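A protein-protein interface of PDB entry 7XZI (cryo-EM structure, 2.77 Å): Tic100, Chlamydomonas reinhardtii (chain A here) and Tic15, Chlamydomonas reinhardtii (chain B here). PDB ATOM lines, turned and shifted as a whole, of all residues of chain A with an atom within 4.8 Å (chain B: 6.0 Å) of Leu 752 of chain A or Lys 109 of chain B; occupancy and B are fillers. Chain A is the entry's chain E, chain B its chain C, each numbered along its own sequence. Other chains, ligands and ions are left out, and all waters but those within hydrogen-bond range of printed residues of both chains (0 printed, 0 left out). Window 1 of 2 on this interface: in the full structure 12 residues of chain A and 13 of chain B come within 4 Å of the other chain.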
ATOM      1  N   TYR A 747     -26.337   8.793  11.631  1.00  0.00           N
ATOM      2  CA  TYR A 747     -25.063   8.401  12.232  1.00  0.00           C
ATOM      3  C   TYR A 747     -24.283   7.591  11.201  1.00  0.00           C
ATOM      4  O   TYR A 747     -24.346   6.359  11.179  1.00  0.00           O
ATOM      5  CB  TYR A 747     -25.276   7.622  13.530  1.00  0.00           C
ATOM      6  CG  TYR A 747     -25.495   8.513  14.732  1.00  0.00           C
ATOM      7  CD1 TYR A 747     -26.764   8.963  15.063  1.00  0.00           C
ATOM      8  CD2 TYR A 747     -24.429   8.909  15.526  1.00  0.00           C
ATOM      9  CE1 TYR A 747     -26.965   9.781  16.157  1.00  0.00           C
ATOM     10  CE2 TYR A 747     -24.622   9.727  16.622  1.00  0.00           C
ATOM     11  CZ  TYR A 747     -25.892  10.160  16.932  1.00  0.00           C
ATOM     12  OH  TYR A 747     -26.091  10.974  18.023  1.00  0.00           O
ATOM     13  N   GLY A 748     -23.543   8.298  10.345  1.00  0.00           N
ATOM     14  CA  GLY A 748     -22.699   7.660   9.359  1.00  0.00           C
ATOM     15  C   GLY A 748     -21.356   8.358   9.290  1.00  0.00           C
ATOM     16  O   GLY A 748     -21.187   9.471   9.790  1.00  0.00           O
ATOM     17  N   GLU A 749     -20.400   7.685   8.646  1.00  0.00           N
ATOM     18  CA  GLU A 749     -19.029   8.185   8.625  1.00  0.00           C
ATOM     19  C   GLU A 749     -18.943   9.550   7.952  1.00  0.00           C
ATOM     20  O   GLU A 749     -18.280  10.462   8.458  1.00  0.00           O
ATOM     21  CB  GLU A 749     -18.118   7.175   7.926  1.00  0.00           C
ATOM     22  CG  GLU A 749     -18.020   5.835   8.637  1.00  0.00           C
ATOM     23  CD  GLU A 749     -17.321   5.936   9.980  1.00  0.00           C
ATOM     24  OE1 GLU A 749     -16.507   6.864  10.164  1.00  0.00           O
ATOM     25  OE2 GLU A 749     -17.589   5.084  10.854  1.00  0.00           O
ATOM     26  N   VAL A 750     -19.614   9.711   6.809  1.00  0.00           N
ATOM     27  CA  VAL A 750     -19.570  10.990   6.105  1.00  0.00           C
ATOM     28  C   VAL A 750     -20.206  12.085   6.950  1.00  0.00           C
ATOM     29  O   VAL A 750     -19.670  13.193   7.062  1.00  0.00           O
ATOM     30  CB  VAL A 750     -20.248  10.878   4.729  1.00  0.00           C
ATOM     31  CG1 VAL A 750     -19.879  12.074   3.867  1.00  0.00           C
ATOM     32  CG2 VAL A 750     -19.857   9.583   4.044  1.00  0.00           C
ATOM     33  N   GLY A 751     -21.357  11.795   7.556  1.00  0.00           N
ATOM     34  CA  GLY A 751     -22.011  12.793   8.387  1.00  0.00           C
ATOM     35  C   GLY A 751     -21.202  13.155   9.617  1.00  0.00           C
ATOM     36  O   GLY A 751     -21.140  14.323  10.009  1.00  0.00           O
ATOM     37  N   LEU A 752     -20.575  12.159  10.247  1.00  0.00           N
ATOM     38  CA  LEU A 752     -19.794  12.417  11.454  1.00  0.00           C
ATOM     39  C   LEU A 752     -18.498  13.159  11.152  1.00  0.00           C
ATOM     40  O   LEU A 752     -18.028  13.941  11.985  1.00  0.00           O
ATOM     41  CB  LEU A 752     -19.487  11.105  12.176  1.00  0.00           C
ATOM     42  CG  LEU A 752     -20.668  10.331  12.762  1.00  0.00           C
ATOM     43  CD1 LEU A 752     -20.198   9.060  13.454  1.00  0.00           C
ATOM     44  CD2 LEU A 752     -21.457  11.207  13.716  1.00  0.00           C
ATOM     45  N   ARG A 753     -17.902  12.927   9.980  1.00  0.00           N
ATOM     46  CA  ARG A 753     -16.561  13.417   9.699  1.00  0.00           C
ATOM     47  C   ARG A 753     -16.501  14.583   8.722  1.00  0.00           C
ATOM     48  O   ARG A 753     -15.427  15.170   8.564  1.00  0.00           O
ATOM     49  CB  ARG A 753     -15.688  12.275   9.158  1.00  0.00           C
ATOM     50  CG  ARG A 753     -15.472  11.145  10.152  1.00  0.00           C
ATOM     51  CD  ARG A 753     -14.839   9.933   9.492  1.00  0.00           C
ATOM     52  NE  ARG A 753     -13.566  10.254   8.865  1.00  0.00           N
ATOM     53  CZ  ARG A 753     -12.814   9.382   8.202  1.00  0.00           C
ATOM     54  NH1 ARG A 753     -13.181   8.119   8.063  1.00  0.00           N
ATOM     55  NH2 ARG A 753     -11.668   9.789   7.668  1.00  0.00           N
ATOM     56  N   MET A 754     -17.608  14.937   8.069  1.00  0.00           N
ATOM     57  CA  MET A 754     -17.599  15.986   7.060  1.00  0.00           C
ATOM     58  C   MET A 754     -18.560  17.130   7.352  1.00  0.00           C
ATOM     59  O   MET A 754     -18.597  18.096   6.583  1.00  0.00           O
ATOM     60  CB  MET A 754     -17.919  15.394   5.681  1.00  0.00           C
ATOM     61  CG  MET A 754     -16.887  14.390   5.190  1.00  0.00           C
ATOM     62  SD  MET A 754     -15.237  15.110   5.079  1.00  0.00           S
ATOM     63  CE  MET A 754     -14.278  13.702   4.522  1.00  0.00           C
ATOM     64  N   PRO A 762     -16.460  19.444  14.751  1.00  0.00           N
ATOM     65  CA  PRO A 762     -17.734  18.783  14.452  1.00  0.00           C
ATOM     66  C   PRO A 762     -18.903  19.497  15.112  1.00  0.00           C
ATOM     67  O   PRO A 762     -18.761  20.144  16.150  1.00  0.00           O
ATOM     68  CB  PRO A 762     -17.545  17.372  15.022  1.00  0.00           C
ATOM     69  CG  PRO A 762     -16.478  17.522  16.052  1.00  0.00           C
ATOM     70  CD  PRO A 762     -15.559  18.579  15.529  1.00  0.00           C
ATOM     71  N   VAL A 763     -20.072  19.374  14.489  1.00  0.00           N
ATOM     72  CA  VAL A 763     -21.295  19.991  14.983  1.00  0.00           C
ATOM     73  C   VAL A 763     -22.309  18.897  15.286  1.00  0.00           C
ATOM     74  O   VAL A 763     -22.274  17.811  14.700  1.00  0.00           O
ATOM     75  CB  VAL A 763     -21.874  21.008  13.976  1.00  0.00           C
ATOM     76  CG1 VAL A 763     -20.913  22.168  13.783  1.00  0.00           C
ATOM     77  CG2 VAL A 763     -22.166  20.329  12.647  1.00  0.00           C
ATOM     78  N   LEU B  86     -18.837  17.710  24.767  1.00  0.00           N
ATOM     79  CA  LEU B  86     -18.766  16.510  23.944  1.00  0.00           C
ATOM     80  C   LEU B  86     -18.688  15.267  24.818  1.00  0.00           C
ATOM     81  O   LEU B  86     -17.997  15.254  25.840  1.00  0.00           O
ATOM     82  CB  LEU B  86     -17.556  16.564  23.011  1.00  0.00           C
ATOM     83  CG  LEU B  86     -17.491  17.745  22.043  1.00  0.00           C
ATOM     84  CD1 LEU B  86     -16.176  17.750  21.280  1.00  0.00           C
ATOM     85  CD2 LEU B  86     -18.667  17.706  21.083  1.00  0.00           C
ATOM     86  N   LEU B  87     -19.404  14.223  24.409  1.00  0.00           N
ATOM     87  CA  LEU B  87     -19.359  12.940  25.100  1.00  0.00           C
ATOM     88  C   LEU B  87     -18.114  12.175  24.669  1.00  0.00           C
ATOM     89  O   LEU B  87     -17.927  11.902  23.479  1.00  0.00           O
ATOM     90  CB  LEU B  87     -20.619  12.130  24.803  1.00  0.00           C
ATOM     91  CG  LEU B  87     -21.915  12.621  25.450  1.00  0.00           C
ATOM     92  CD1 LEU B  87     -23.115  11.875  24.894  1.00  0.00           C
ATOM     93  CD2 LEU B  87     -21.837  12.454  26.955  1.00  0.00           C
ATOM     94  N   TRP B  98      -7.459  14.511  10.556  1.00  0.00           N
ATOM     95  CA  TRP B  98      -8.571  15.055  11.321  1.00  0.00           C
ATOM     96  C   TRP B  98      -9.205  14.037  12.255  1.00  0.00           C
ATOM     97  O   TRP B  98      -9.750  14.421  13.294  1.00  0.00           O
ATOM     98  CB  TRP B  98      -9.645  15.603  10.375  1.00  0.00           C
ATOM     99  CG  TRP B  98     -10.760  16.312  11.076  1.00  0.00           C
ATOM    100  CD1 TRP B  98     -10.811  17.636  11.397  1.00  0.00           C
ATOM    101  CD2 TRP B  98     -11.988  15.740  11.541  1.00  0.00           C
ATOM    102  NE1 TRP B  98     -11.993  17.924  12.033  1.00  0.00           N
ATOM    103  CE2 TRP B  98     -12.733  16.777  12.136  1.00  0.00           C
ATOM    104  CE3 TRP B  98     -12.528  14.451  11.515  1.00  0.00           C
ATOM    105  CZ2 TRP B  98     -13.990  16.566  12.699  1.00  0.00           C
ATOM    106  CZ3 TRP B  98     -13.776  14.243  12.074  1.00  0.00           C
ATOM    107  CH2 TRP B  98     -14.493  15.295  12.657  1.00  0.00           C
ATOM    108  N   ASN B 104     -11.815  10.877  20.413  1.00  0.00           N
ATOM    109  CA  ASN B 104     -12.667  10.481  21.534  1.00  0.00           C
ATOM    110  C   ASN B 104     -14.148  10.596  21.181  1.00  0.00           C
ATOM    111  O   ASN B 104     -14.931   9.665  21.414  1.00  0.00           O
ATOM    112  CB  ASN B 104     -12.340  11.328  22.764  1.00  0.00           C
ATOM    113  CG  ASN B 104     -10.911  11.143  23.240  1.00  0.00           C
ATOM    114  OD1 ASN B 104     -10.346  10.054  23.147  1.00  0.00           O
ATOM    115  ND2 ASN B 104     -10.318  12.213  23.755  1.00  0.00           N
ATOM    116  N   ASN B 105     -14.557  11.742  20.627  1.00  0.00           N
ATOM    117  CA  ASN B 105     -15.961  11.930  20.275  1.00  0.00           C
ATOM    118  C   ASN B 105     -16.384  10.976  19.163  1.00  0.00           C
ATOM    119  O   ASN B 105     -17.496  10.439  19.189  1.00  0.00           O
ATOM    120  CB  ASN B 105     -16.216  13.381  19.867  1.00  0.00           C
ATOM    121  CG  ASN B 105     -17.693  13.736  19.864  1.00  0.00           C
ATOM    122  OD1 ASN B 105     -18.505  13.066  20.502  1.00  0.00           O
ATOM    123  ND2 ASN B 105     -18.047  14.795  19.145  1.00  0.00           N
ATOM    124  N   LEU B 106     -15.510  10.757  18.177  1.00  0.00           N
ATOM    125  CA  LEU B 106     -15.813   9.794  17.122  1.00  0.00           C
ATOM    126  C   LEU B 106     -15.940   8.385  17.684  1.00  0.00           C
ATOM    127  O   LEU B 106     -16.809   7.617  17.260  1.00  0.00           O
ATOM    128  CB  LEU B 106     -14.741   9.847  16.034  1.00  0.00           C
ATOM    129  CG  LEU B 106     -15.034  10.766  14.849  1.00  0.00           C
ATOM    130  CD1 LEU B 106     -13.871  10.775  13.874  1.00  0.00           C
ATOM    131  CD2 LEU B 106     -16.310  10.323  14.156  1.00  0.00           C
ATOM    132  N   HIS B 107     -15.075   8.025  18.635  1.00  0.00           N
ATOM    133  CA  HIS B 107     -15.166   6.715  19.268  1.00  0.00           C
ATOM    134  C   HIS B 107     -16.484   6.556  20.011  1.00  0.00           C
ATOM    135  O   HIS B 107     -17.107   5.489  19.968  1.00  0.00           O
ATOM    136  CB  HIS B 107     -13.986   6.511  20.217  1.00  0.00           C
ATOM    137  CG  HIS B 107     -14.066   5.252  21.023  1.00  0.00           C
ATOM    138  ND1 HIS B 107     -13.905   4.001  20.468  1.00  0.00           N
ATOM    139  CD2 HIS B 107     -14.296   5.051  22.342  1.00  0.00           C
ATOM    140  CE1 HIS B 107     -14.029   3.085  21.409  1.00  0.00           C
ATOM    141  NE2 HIS B 107     -14.268   3.694  22.555  1.00  0.00           N
ATOM    142  N   TRP B 108     -16.919   7.606  20.711  1.00  0.00           N
ATOM    143  CA  TRP B 108     -18.213   7.549  21.385  1.00  0.00           C
ATOM    144  C   TRP B 108     -19.356   7.412  20.385  1.00  0.00           C
ATOM    145  O   TRP B 108     -20.288   6.628  20.599  1.00  0.00           O
ATOM    146  CB  TRP B 108     -18.414   8.785  22.259  1.00  0.00           C
ATOM    147  CG  TRP B 108     -19.817   8.920  22.770  1.00  0.00           C
ATOM    148  CD1 TRP B 108     -20.837   9.616  22.189  1.00  0.00           C
ATOM    149  CD2 TRP B 108     -20.359   8.335  23.960  1.00  0.00           C
ATOM    150  NE1 TRP B 108     -21.978   9.504  22.943  1.00  0.00           N
ATOM    151  CE2 TRP B 108     -21.711   8.724  24.037  1.00  0.00           C
ATOM    152  CE3 TRP B 108     -19.832   7.524  24.969  1.00  0.00           C
ATOM    153  CZ2 TRP B 108     -22.543   8.329  25.082  1.00  0.00           C
ATOM    154  CZ3 TRP B 108     -20.659   7.134  26.006  1.00  0.00           C
ATOM    155  CH2 TRP B 108     -22.000   7.536  26.055  1.00  0.00           C
ATOM    156  N   LYS B 109     -19.305   8.170  19.288  1.00  0.00           N
ATOM    157  CA  LYS B 109     -20.420   8.187  18.347  1.00  0.00           C
ATOM    158  C   LYS B 109     -20.481   6.924  17.498  1.00  0.00           C
ATOM    159  O   LYS B 109     -21.559   6.554  17.023  1.00  0.00           O
ATOM    160  CB  LYS B 109     -20.333   9.422  17.452  1.00  0.00           C
ATOM    161  CG  LYS B 109     -20.633  10.722  18.170  1.00  0.00           C
ATOM    162  CD  LYS B 109     -20.653  11.891  17.205  1.00  0.00           C
ATOM    163  CE  LYS B 109     -21.105  13.164  17.897  1.00  0.00           C
ATOM    164  NZ  LYS B 109     -21.186  14.309  16.951  1.00  0.00           N
ATOM    165  N   ARG B 110     -19.345   6.257  17.287  1.00  0.00           N
ATOM    166  CA  ARG B 110     -19.319   5.066  16.447  1.00  0.00           C
ATOM    167  C   ARG B 110     -19.996   3.865  17.088  1.00  0.00           C
ATOM    168  O   ARG B 110     -20.234   2.870  16.395  1.00  0.00           O
ATOM    169  CB  ARG B 110     -17.874   4.715  16.088  1.00  0.00           C
ATOM    170  CG  ARG B 110     -17.310   5.532  14.939  1.00  0.00           C
ATOM    171  CD  ARG B 110     -15.801   5.386  14.844  1.00  0.00           C
ATOM    172  NE  ARG B 110     -15.260   6.057  13.671  1.00  0.00           N
ATOM    173  CZ  ARG B 110     -13.964   6.224  13.435  1.00  0.00           C
ATOM    174  NH1 ARG B 110     -13.046   5.796  14.287  1.00  0.00           N
ATOM    175  NH2 ARG B 110     -13.582   6.837  12.320  1.00  0.00           N
ATOM    176  N   TRP B 111     -20.310   3.924  18.381  1.00  0.00           N
ATOM    177  CA  TRP B 111     -20.997   2.843  19.072  1.00  0.00           C
ATOM    178  C   TRP B 111     -22.486   3.114  19.243  1.00  0.00           C
ATOM    179  O   TRP B 111     -23.095   2.604  20.187  1.00  0.00           O
ATOM    180  CB  TRP B 111     -20.356   2.592  20.438  1.00  0.00           C
ATOM    181  CG  TRP B 111     -19.028   1.912  20.374  1.00  0.00           C
ATOM    182  CD1 TRP B 111     -17.800   2.497  20.461  1.00  0.00           C
ATOM    183  CD2 TRP B 111     -18.792   0.508  20.218  1.00  0.00           C
ATOM    184  NE1 TRP B 111     -16.813   1.547  20.364  1.00  0.00           N
ATOM    185  CE2 TRP B 111     -17.397   0.317  20.216  1.00  0.00           C
ATOM    186  CE3 TRP B 111     -19.627  -0.604  20.079  1.00  0.00           C
ATOM    187  CZ2 TRP B 111     -16.817  -0.942  20.078  1.00  0.00           C
ATOM    188  CZ3 TRP B 111     -19.050  -1.852  19.943  1.00  0.00           C
ATOM    189  CH2 TRP B 111     -17.658  -2.011  19.943  1.00  0.00           C
ATOM    190  N   LYS B 112     -23.084   3.908  18.352  1.00  0.00           N
ATOM    191  CA  LYS B 112     -24.474   4.315  18.541  1.00  0.00           C
ATOM    192  C   LYS B 112     -25.425   3.128  18.433  1.00  0.00           C
ATOM    193  O   LYS B 112     -26.279   2.925  19.302  1.00  0.00           O
ATOM    194  CB  LYS B 112     -24.848   5.395  17.527  1.00  0.00           C
ATOM    195  CG  LYS B 112     -26.253   5.947  17.706  1.00  0.00           C
ATOM    196  CD  LYS B 112     -26.423   6.597  19.069  1.00  0.00           C
ATOM    197  CE  LYS B 112     -27.780   7.267  19.197  1.00  0.00           C
ATOM    198  NZ  LYS B 112     -28.894   6.301  18.991  1.00  0.00           N
ATOM    199  N   VAL B 113     -25.301   2.341  17.369  1.00  0.00           N
ATOM    200  CA  VAL B 113     -26.199   1.210  17.140  1.00  0.00           C
ATOM    201  C   VAL B 113     -26.041   0.143  18.223  1.00  0.00           C
ATOM    202  O   VAL B 113     -27.056  -0.289  18.791  1.00  0.00           O
ATOM    203  CB  VAL B 113     -25.993   0.615  15.737  1.00  0.00           C
ATOM    204  CG1 VAL B 113     -26.909  -0.578  15.530  1.00  0.00           C
ATOM    205  CG2 VAL B 113     -26.242   1.674  14.676  1.00  0.00           C
ATOM    206  N   ARG B 115     -24.992   0.423  21.283  1.00  0.00           N
ATOM    207  CA  ARG B 115     -25.345   0.926  22.607  1.00  0.00           C
ATOM    208  C   ARG B 115     -26.854   0.922  22.825  1.00  0.00           C
ATOM    209  O   ARG B 115     -27.327   0.619  23.925  1.00  0.00           O
ATOM    210  CB  ARG B 115     -24.775   2.332  22.801  1.00  0.00           C
ATOM    211  CG  ARG B 115     -25.157   2.991  24.116  1.00  0.00           C
ATOM    212  CD  ARG B 115     -24.332   4.243  24.393  1.00  0.00           C
ATOM    213  NE  ARG B 115     -24.444   5.237  23.335  1.00  0.00           N
ATOM    214  CZ  ARG B 115     -23.483   5.512  22.459  1.00  0.00           C
ATOM    215  NH1 ARG B 115     -22.316   4.892  22.497  1.00  0.00           N
ATOM    216  NH2 ARG B 115     -23.701   6.432  21.524  1.00  0.00           N
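The guanidinium group (NH2) of Arg 110 of chain B is in salt-bridge range of the side-chain carboxylate (OE1) of Glu 749 of chain A (3.6 Å).
Among the printed residues, pairs that only touch across the chains: Leu 752 of chain A with Lys 109 of chain B (3.6 Å), Arg 753 of chain A with Trp 98 of chain B (3.8 Å), Pro 762 of chain A with Trp 98 of chain B (3.8 Å), Leu 752 of chain A with Leu 106 of chain B (3.8 Å) and Leu 752 of chain A with Trp 98 of chain B (3.8 Å).
Printed residues of chain B within 4 Å of Glu 749 of chain A: Arg 110 (3.6 Å). Leu 752 of chain A touches just these residues of chain B: Trp 98 (3.8 Å), Leu 106 (3.8 Å) and Lys 109 (3.6 Å). Of the printed residues of chain A, Lys 109 of chain B touches Leu 752. Of the printed residues of chain A, Arg 110 of chain B touches Glu 749. Lys 112 of chain B touches none of the printed residues of chain A. The nearest printed residue of chain A that does not touch Lys 109 of chain B is Tyr 747 of chain A (4.003 Å). The nearest printed residue of chain A that does not touch Arg 110 of chain B is Arg 753 of chain A (4.4 Å).
Of the 14 printed residues of chain B, 4 touch a printed residue of chain A. Printed residues of chain B that touch a printed residue of chain A: Trp 98, Leu 106, Lys 109 and Arg 110. Printed residues of chain A that touch a printed residue of chain B: Glu 749, Leu 752, Arg 753 and Pro 762. Hydrophobic or aromatic side chains of chain A that line the printed part of chain B: Leu 752 and Pro 762. Among the printed residues, Asp or Glu carboxylates within 4 Å of a Lys or Arg side-chain nitrogen of the other chain: Glu 749 of chain A with Arg 110 of chain B.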
